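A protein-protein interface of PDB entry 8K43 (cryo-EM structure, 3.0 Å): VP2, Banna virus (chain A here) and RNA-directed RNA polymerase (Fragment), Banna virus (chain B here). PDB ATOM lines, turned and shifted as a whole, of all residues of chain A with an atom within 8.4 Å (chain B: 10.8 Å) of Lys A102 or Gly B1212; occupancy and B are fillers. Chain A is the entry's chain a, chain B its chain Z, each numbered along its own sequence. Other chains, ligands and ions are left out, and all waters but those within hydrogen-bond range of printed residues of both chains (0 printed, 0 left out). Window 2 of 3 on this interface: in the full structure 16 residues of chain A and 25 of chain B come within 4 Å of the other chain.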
ATOM      1  N   LYS A  95      18.462  12.456  28.491  1.00  0.00           N
ATOM      2  CA  LYS A  95      17.400  12.144  27.542  1.00  0.00           C
ATOM      3  C   LYS A  95      16.025  12.485  28.102  1.00  0.00           C
ATOM      4  O   LYS A  95      15.115  12.828  27.340  1.00  0.00           O
ATOM      5  CB  LYS A  95      17.463  10.670  27.150  1.00  0.00           C
ATOM      6  CG  LYS A  95      16.689  10.325  25.888  1.00  0.00           C
ATOM      7  CD  LYS A  95      17.071  11.242  24.739  1.00  0.00           C
ATOM      8  CE  LYS A  95      15.898  11.467  23.799  1.00  0.00           C
ATOM      9  NZ  LYS A  95      14.852  12.330  24.415  1.00  0.00           N
ATOM     10  N   GLN A  96      15.852  12.385  29.423  1.00  0.00           N
ATOM     11  CA  GLN A  96      14.555  12.676  30.025  1.00  0.00           C
ATOM     12  C   GLN A  96      14.170  14.139  29.834  1.00  0.00           C
ATOM     13  O   GLN A  96      13.012  14.452  29.531  1.00  0.00           O
ATOM     14  CB  GLN A  96      14.575  12.316  31.510  1.00  0.00           C
ATOM     15  CG  GLN A  96      13.315  11.623  31.998  1.00  0.00           C
ATOM     16  CD  GLN A  96      12.274  12.600  32.508  1.00  0.00           C
ATOM     17  OE1 GLN A  96      12.567  13.462  33.335  1.00  0.00           O
ATOM     18  NE2 GLN A  96      11.048  12.468  32.014  1.00  0.00           N
ATOM     19  N   LYS A  97      15.130  15.051  30.013  1.00  0.00           N
ATOM     20  CA  LYS A  97      14.852  16.467  29.805  1.00  0.00           C
ATOM     21  C   LYS A  97      14.468  16.744  28.358  1.00  0.00           C
ATOM     22  O   LYS A  97      13.528  17.502  28.090  1.00  0.00           O
ATOM     23  CB  LYS A  97      16.066  17.302  30.207  1.00  0.00           C
ATOM     24  CG  LYS A  97      15.880  18.798  30.019  1.00  0.00           C
ATOM     25  CD  LYS A  97      17.174  19.461  29.579  1.00  0.00           C
ATOM     26  CE  LYS A  97      17.556  19.044  28.170  1.00  0.00           C
ATOM     27  NZ  LYS A  97      16.476  19.346  27.191  1.00  0.00           N
ATOM     28  N   LEU A  98      15.182  16.133  27.408  1.00  0.00           N
ATOM     29  CA  LEU A  98      14.854  16.318  26.000  1.00  0.00           C
ATOM     30  C   LEU A  98      13.466  15.781  25.680  1.00  0.00           C
ATOM     31  O   LEU A  98      12.712  16.403  24.925  1.00  0.00           O
ATOM     32  CB  LEU A  98      15.907  15.645  25.122  1.00  0.00           C
ATOM     33  CG  LEU A  98      17.269  16.338  25.063  1.00  0.00           C
ATOM     34  CD1 LEU A  98      18.328  15.401  24.503  1.00  0.00           C
ATOM     35  CD2 LEU A  98      17.186  17.615  24.238  1.00  0.00           C
ATOM     36  N   ASP A  99      13.111  14.622  26.241  1.00  0.00           N
ATOM     37  CA  ASP A  99      11.783  14.067  26.005  1.00  0.00           C
ATOM     38  C   ASP A  99      10.697  14.972  26.572  1.00  0.00           C
ATOM     39  O   ASP A  99       9.678  15.227  25.911  1.00  0.00           O
ATOM     40  CB  ASP A  99      11.687  12.667  26.613  1.00  0.00           C
ATOM     41  CG  ASP A  99      10.254  12.225  26.833  1.00  0.00           C
ATOM     42  OD1 ASP A  99       9.537  12.008  25.833  1.00  0.00           O
ATOM     43  OD2 ASP A  99       9.844  12.094  28.006  1.00  0.00           O
ATOM     44  N   LYS A 100      10.897  15.476  27.792  1.00  0.00           N
ATOM     45  CA  LYS A 100       9.919  16.385  28.379  1.00  0.00           C
ATOM     46  C   LYS A 100       9.776  17.649  27.545  1.00  0.00           C
ATOM     47  O   LYS A 100       8.663  18.155  27.356  1.00  0.00           O
ATOM     48  CB  LYS A 100      10.312  16.730  29.815  1.00  0.00           C
ATOM     49  CG  LYS A 100       9.971  15.652  30.829  1.00  0.00           C
ATOM     50  CD  LYS A 100      10.612  15.933  32.179  1.00  0.00           C
ATOM     51  CE  LYS A 100      10.590  17.417  32.512  1.00  0.00           C
ATOM     52  NZ  LYS A 100       9.234  17.871  32.926  1.00  0.00           N
ATOM     53  N   LEU A 101      10.891  18.182  27.043  1.00  0.00           N
ATOM     54  CA  LEU A 101      10.824  19.374  26.207  1.00  0.00           C
ATOM     55  C   LEU A 101      10.090  19.098  24.899  1.00  0.00           C
ATOM     56  O   LEU A 101       9.264  19.910  24.465  1.00  0.00           O
ATOM     57  CB  LEU A 101      12.230  19.901  25.938  1.00  0.00           C
ATOM     58  CG  LEU A 101      12.648  21.118  26.761  1.00  0.00           C
ATOM     59  CD1 LEU A 101      12.766  20.755  28.231  1.00  0.00           C
ATOM     60  CD2 LEU A 101      13.955  21.693  26.244  1.00  0.00           C
ATOM     61  N   LYS A 102      10.375  17.963  24.257  1.00  0.00           N
ATOM     62  CA  LYS A 102       9.696  17.621  23.013  1.00  0.00           C
ATOM     63  C   LYS A 102       8.212  17.369  23.216  1.00  0.00           C
ATOM     64  O   LYS A 102       7.434  17.504  22.264  1.00  0.00           O
ATOM     65  CB  LYS A 102      10.342  16.393  22.370  1.00  0.00           C
ATOM     66  CG  LYS A 102      11.785  16.595  21.940  1.00  0.00           C
ATOM     67  CD  LYS A 102      11.882  17.533  20.750  1.00  0.00           C
ATOM     68  CE  LYS A 102      13.318  17.667  20.270  1.00  0.00           C
ATOM     69  NZ  LYS A 102      13.949  18.927  20.748  1.00  0.00           N
ATOM     70  N   LEU A 103       7.805  16.983  24.428  1.00  0.00           N
ATOM     71  CA  LEU A 103       6.383  16.845  24.712  1.00  0.00           C
ATOM     72  C   LEU A 103       5.637  18.153  24.487  1.00  0.00           C
ATOM     73  O   LEU A 103       4.468  18.140  24.088  1.00  0.00           O
ATOM     74  CB  LEU A 103       6.172  16.361  26.145  1.00  0.00           C
ATOM     75  CG  LEU A 103       5.057  15.338  26.370  1.00  0.00           C
ATOM     76  CD1 LEU A 103       4.895  14.430  25.163  1.00  0.00           C
ATOM     77  CD2 LEU A 103       5.327  14.524  27.625  1.00  0.00           C
ATOM     78  N   PHE A 104       6.290  19.290  24.738  1.00  0.00           N
ATOM     79  CA  PHE A 104       5.634  20.578  24.548  1.00  0.00           C
ATOM     80  C   PHE A 104       5.303  20.820  23.083  1.00  0.00           C
ATOM     81  O   PHE A 104       4.260  21.402  22.763  1.00  0.00           O
ATOM     82  CB  PHE A 104       6.515  21.705  25.081  1.00  0.00           C
ATOM     83  CG  PHE A 104       6.255  22.046  26.516  1.00  0.00           C
ATOM     84  CD1 PHE A 104       5.222  22.894  26.861  1.00  0.00           C
ATOM     85  CD2 PHE A 104       7.047  21.520  27.518  1.00  0.00           C
ATOM     86  CE1 PHE A 104       4.978  23.210  28.181  1.00  0.00           C
ATOM     87  CE2 PHE A 104       6.810  21.832  28.839  1.00  0.00           C
ATOM     88  CZ  PHE A 104       5.775  22.676  29.171  1.00  0.00           C
ATOM     89  N   GLU A 105       6.177  20.385  22.180  1.00  0.00           N
ATOM     90  CA  GLU A 105       6.001  20.654  20.761  1.00  0.00           C
ATOM     91  C   GLU A 105       5.261  19.550  20.020  1.00  0.00           C
ATOM     92  O   GLU A 105       4.746  19.800  18.925  1.00  0.00           O
ATOM     93  CB  GLU A 105       7.367  20.893  20.106  1.00  0.00           C
ATOM     94  CG  GLU A 105       7.942  19.696  19.375  1.00  0.00           C
ATOM     95  CD  GLU A 105       9.201  20.043  18.605  1.00  0.00           C
ATOM     96  OE1 GLU A 105       9.763  21.132  18.844  1.00  0.00           O
ATOM     97  OE2 GLU A 105       9.631  19.225  17.764  1.00  0.00           O
ATOM     98  N   THR A 106       5.184  18.344  20.582  1.00  0.00           N
ATOM     99  CA  THR A 106       4.487  17.256  19.910  1.00  0.00           C
ATOM    100  C   THR A 106       2.971  17.396  19.955  1.00  0.00           C
ATOM    101  O   THR A 106       2.278  16.656  19.249  1.00  0.00           O
ATOM    102  CB  THR A 106       4.895  15.911  20.520  1.00  0.00           C
ATOM    103  OG1 THR A 106       4.746  14.876  19.539  1.00  0.00           O
ATOM    104  CG2 THR A 106       4.035  15.584  21.731  1.00  0.00           C
ATOM    105  N   SER A 107       2.440  18.315  20.757  1.00  0.00           N
ATOM    106  CA  SER A 107       1.005  18.505  20.890  1.00  0.00           C
ATOM    107  C   SER A 107       0.735  19.982  21.126  1.00  0.00           C
ATOM    108  O   SER A 107       1.610  20.694  21.629  1.00  0.00           O
ATOM    109  CB  SER A 107       0.439  17.668  22.048  1.00  0.00           C
ATOM    110  OG  SER A 107       0.201  16.332  21.638  1.00  0.00           O
ATOM    111  N   TYR B1037       9.271  27.849  33.426  1.00  0.00           N
ATOM    112  CA  TYR B1037      10.618  28.116  32.945  1.00  0.00           C
ATOM    113  C   TYR B1037      10.911  29.604  33.073  1.00  0.00           C
ATOM    114  O   TYR B1037      10.084  30.436  32.692  1.00  0.00           O
ATOM    115  CB  TYR B1037      10.775  27.640  31.502  1.00  0.00           C
ATOM    116  CG  TYR B1037      10.477  26.167  31.338  1.00  0.00           C
ATOM    117  CD1 TYR B1037       9.189  25.722  31.092  1.00  0.00           C
ATOM    118  CD2 TYR B1037      11.485  25.220  31.449  1.00  0.00           C
ATOM    119  CE1 TYR B1037       8.913  24.378  30.952  1.00  0.00           C
ATOM    120  CE2 TYR B1037      11.218  23.874  31.310  1.00  0.00           C
ATOM    121  CZ  TYR B1037       9.930  23.459  31.060  1.00  0.00           C
ATOM    122  OH  TYR B1037       9.658  22.119  30.921  1.00  0.00           O
ATOM    123  N   HIS B1207       6.498  27.761  28.893  1.00  0.00           N
ATOM    124  CA  HIS B1207       7.077  27.114  27.728  1.00  0.00           C
ATOM    125  C   HIS B1207       8.573  27.380  27.686  1.00  0.00           C
ATOM    126  O   HIS B1207       8.996  28.515  27.945  1.00  0.00           O
ATOM    127  CB  HIS B1207       6.420  27.615  26.439  1.00  0.00           C
ATOM    128  CG  HIS B1207       6.791  26.830  25.221  1.00  0.00           C
ATOM    129  ND1 HIS B1207       8.052  26.871  24.666  1.00  0.00           N
ATOM    130  CD2 HIS B1207       6.065  25.995  24.443  1.00  0.00           C
ATOM    131  CE1 HIS B1207       8.088  26.088  23.604  1.00  0.00           C
ATOM    132  NE2 HIS B1207       6.895  25.547  23.444  1.00  0.00           N
ATOM    133  N   PRO B1208       9.387  26.376  27.373  1.00  0.00           N
ATOM    134  CA  PRO B1208      10.836  26.589  27.323  1.00  0.00           C
ATOM    135  C   PRO B1208      11.233  27.530  26.200  1.00  0.00           C
ATOM    136  O   PRO B1208      10.552  27.647  25.178  1.00  0.00           O
ATOM    137  CB  PRO B1208      11.394  25.182  27.085  1.00  0.00           C
ATOM    138  CG  PRO B1208      10.304  24.257  27.488  1.00  0.00           C
ATOM    139  CD  PRO B1208       9.034  24.964  27.162  1.00  0.00           C
ATOM    140  N   SER B1209      12.360  28.211  26.405  1.00  0.00           N
ATOM    141  CA  SER B1209      12.861  29.145  25.408  1.00  0.00           C
ATOM    142  C   SER B1209      13.524  28.437  24.233  1.00  0.00           C
ATOM    143  O   SER B1209      13.474  28.941  23.107  1.00  0.00           O
ATOM    144  CB  SER B1209      13.848  30.118  26.047  1.00  0.00           C
ATOM    145  OG  SER B1209      14.782  29.431  26.859  1.00  0.00           O
ATOM    146  N   LYS B1210      14.146  27.283  24.468  1.00  0.00           N
ATOM    147  CA  LYS B1210      14.871  26.545  23.435  1.00  0.00           C
ATOM    148  C   LYS B1210      14.503  25.068  23.540  1.00  0.00           C
ATOM    149  O   LYS B1210      15.167  24.307  24.246  1.00  0.00           O
ATOM    150  CB  LYS B1210      16.373  26.758  23.580  1.00  0.00           C
ATOM    151  CG  LYS B1210      17.129  26.773  22.265  1.00  0.00           C
ATOM    152  CD  LYS B1210      18.623  26.917  22.495  1.00  0.00           C
ATOM    153  CE  LYS B1210      19.396  26.710  21.208  1.00  0.00           C
ATOM    154  NZ  LYS B1210      19.623  27.995  20.492  1.00  0.00           N
ATOM    155  N   ILE B1211      13.444  24.664  22.836  1.00  0.00           N
ATOM    156  CA  ILE B1211      13.058  23.256  22.831  1.00  0.00           C
ATOM    157  C   ILE B1211      14.074  22.432  22.054  1.00  0.00           C
ATOM    158  O   ILE B1211      14.536  21.383  22.519  1.00  0.00           O
ATOM    159  CB  ILE B1211      11.640  23.087  22.258  1.00  0.00           C
ATOM    160  CG1 ILE B1211      10.594  23.341  23.344  1.00  0.00           C
ATOM    161  CG2 ILE B1211      11.463  21.698  21.669  1.00  0.00           C
ATOM    162  CD1 ILE B1211       9.201  22.892  22.960  1.00  0.00           C
ATOM    163  N   GLY B1212      14.444  22.897  20.866  1.00  0.00           N
ATOM    164  CA  GLY B1212      15.417  22.202  20.052  1.00  0.00           C
ATOM    165  C   GLY B1212      16.705  22.982  19.927  1.00  0.00           C
ATOM    166  O   GLY B1212      16.728  24.192  20.172  1.00  0.00           O
ATOM    167  N   ASN B1213      17.790  22.302  19.552  1.00  0.00           N
ATOM    168  CA  ASN B1213      19.065  22.984  19.372  1.00  0.00           C
ATOM    169  C   ASN B1213      18.993  24.042  18.280  1.00  0.00           C
ATOM    170  O   ASN B1213      19.795  24.982  18.285  1.00  0.00           O
ATOM    171  CB  ASN B1213      20.163  21.965  19.056  1.00  0.00           C
ATOM    172  CG  ASN B1213      21.504  22.615  18.780  1.00  0.00           C
ATOM    173  OD1 ASN B1213      22.144  23.154  19.684  1.00  0.00           O
ATOM    174  ND2 ASN B1213      21.939  22.568  17.526  1.00  0.00           N
ATOM    175  N   THR B1214      18.043  23.918  17.357  1.00  0.00           N
ATOM    176  CA  THR B1214      17.867  24.874  16.274  1.00  0.00           C
ATOM    177  C   THR B1214      16.760  25.883  16.539  1.00  0.00           C
ATOM    178  O   THR B1214      16.890  27.052  16.166  1.00  0.00           O
ATOM    179  CB  THR B1214      17.573  24.136  14.965  1.00  0.00           C
ATOM    180  OG1 THR B1214      16.192  23.754  14.933  1.00  0.00           O
ATOM    181  CG2 THR B1214      18.436  22.892  14.854  1.00  0.00           C
ATOM    182  N   VAL B1215      15.682  25.467  17.183  1.00  0.00           N
ATOM    183  CA  VAL B1215      14.494  26.299  17.334  1.00  0.00           C
ATOM    184  C   VAL B1215      14.572  27.090  18.633  1.00  0.00           C
ATOM    185  O   VAL B1215      15.128  26.628  19.636  1.00  0.00           O
ATOM    186  CB  VAL B1215      13.221  25.434  17.266  1.00  0.00           C
ATOM    187  CG1 VAL B1215      13.008  24.682  18.561  1.00  0.00           C
ATOM    188  CG2 VAL B1215      12.007  26.296  16.951  1.00  0.00           C
ATOM    189  N   TYR B1216      14.040  28.309  18.598  1.00  0.00           N
ATOM    190  CA  TYR B1216      13.954  29.184  19.758  1.00  0.00           C
ATOM    191  C   TYR B1216      12.558  29.784  19.807  1.00  0.00           C
ATOM    192  O   TYR B1216      12.037  30.244  18.788  1.00  0.00           O
ATOM    193  CB  TYR B1216      15.020  30.286  19.699  1.00  0.00           C
ATOM    194  CG  TYR B1216      14.640  31.570  20.398  1.00  0.00           C
ATOM    195  CD1 TYR B1216      14.057  32.621  19.699  1.00  0.00           C
ATOM    196  CD2 TYR B1216      14.871  31.737  21.755  1.00  0.00           C
ATOM    197  CE1 TYR B1216      13.711  33.798  20.336  1.00  0.00           C
ATOM    198  CE2 TYR B1216      14.528  32.911  22.402  1.00  0.00           C
ATOM    199  CZ  TYR B1216      13.948  33.938  21.686  1.00  0.00           C
ATOM    200  OH  TYR B1216      13.606  35.106  22.327  1.00  0.00           O
ATOM    201  N   TYR B1217      11.955  29.783  20.992  1.00  0.00           N
ATOM    202  CA  TYR B1217      10.562  30.166  21.150  1.00  0.00           C
ATOM    203  C   TYR B1217      10.431  31.510  21.850  1.00  0.00           C
ATOM    204  O   TYR B1217      11.292  31.909  22.638  1.00  0.00           O
ATOM    205  CB  TYR B1217       9.780  29.107  21.928  1.00  0.00           C
ATOM    206  CG  TYR B1217       9.515  27.844  21.148  1.00  0.00           C
ATOM    207  CD1 TYR B1217       8.244  27.556  20.674  1.00  0.00           C
ATOM    208  CD2 TYR B1217      10.524  26.933  20.898  1.00  0.00           C
ATOM    209  CE1 TYR B1217       7.991  26.403  19.964  1.00  0.00           C
ATOM    210  CE2 TYR B1217      10.280  25.781  20.194  1.00  0.00           C
ATOM    211  CZ  TYR B1217       9.015  25.518  19.727  1.00  0.00           C
ATOM    212  OH  TYR B1217       8.776  24.363  19.020  1.00  0.00           O
ATOM    213  N   ASP B1218       9.337  32.205  21.547  1.00  0.00           N
ATOM    214  CA  ASP B1218       9.019  33.478  22.176  1.00  0.00           C
ATOM    215  C   ASP B1218       7.523  33.550  22.435  1.00  0.00           C
ATOM    216  O   ASP B1218       6.720  33.007  21.675  1.00  0.00           O
ATOM    217  CB  ASP B1218       9.460  34.664  21.315  1.00  0.00           C
ATOM    218  CG  ASP B1218       8.984  34.553  19.884  1.00  0.00           C
ATOM    219  OD1 ASP B1218       8.486  33.472  19.504  1.00  0.00           O
ATOM    220  OD2 ASP B1218       9.104  35.545  19.139  1.00  0.00           O
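The backbone carbonyl oxygen (O) of Ile B1211 is in hydrogen-bond range of the side-chain amino group (NZ) of Lys A102, at 3.1 Å. The side-chain hydroxyl (OH) of Tyr B1217 sits at hydrogen-bond distance from the side-chain carboxylate (OE1) of Glu A105, at 3.4 Å.
The backbone NH (N) of Tyr B1217 is in hydrogen-bond range of the backbone carbonyl oxygen (O) of Ser B1209, at 2.7 Å.
Pro B1208 touches Leu A101 (CG to CG, 3.98 Å). Lys B1210 touches Leu A101 (O to CD2, 3.5 Å). Ile B1211 touches Leu A101 (CD1 to O, 3.3 Å). NZ of Lys A102 touches CA of Gly B1212, 3.7 Å away. Phe A104 touches Tyr B1037. CD2 of Phe A104 touches CD of Pro B1208 (3.99 Å). CB of Phe A104 touches CD1 of Ile B1211, 3.6 Å away. Ile B1211 touches Glu A105.
Of chain B, only Ile B1211 (3.1 Å) and Gly B1212 (3.7 Å) come within 4 Å of Lys A102. Of chain A, only Lys A102 (3.7 Å) comes within 4 Å of Gly B1212. Leu A103 touches none of the printed residues of chain B. No residue of chain B comes within 4 Å of Thr A106. Of the printed residues of chain A, Tyr B1217 touches Glu A105 (3.4 Å). Of the printed residues of chain A, Tyr B1037 touches Phe A104 (3.5 Å). Printed residues of chain A within 4 Å of Pro B1208: Leu A101 (3.98 Å) and Phe A104 (3.99 Å). Of the printed residues of chain A, Ile B1211 touches Leu A101 (3.3 Å), Lys A102 (3.1 Å), Phe A104 (3.6 Å) and Glu A105 (3.3 Å). Gln A96 touches none of the printed residues of chain B.
Of the 13 printed residues of chain B, 6 touch a printed residue of chain A. Printed residues of chain B that touch a printed residue of chain A: Tyr B1037, Pro B1208, Lys B1210, Ile B1211, Gly B1212 and Tyr B1217. Hydrophobic or aromatic side chains of chain B within 4 Å of the printed part of chain A: Tyr B1037, Pro B1208, Ile B1211 and Tyr B1217. Printed residues of chain A that touch a printed residue of chain B: Leu A101, Lys A102, Phe A104 and Glu A105. Hydrophobic or aromatic side chains of chain A within 4 Å of the printed part of chain B: Leu A101 and Phe A104.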
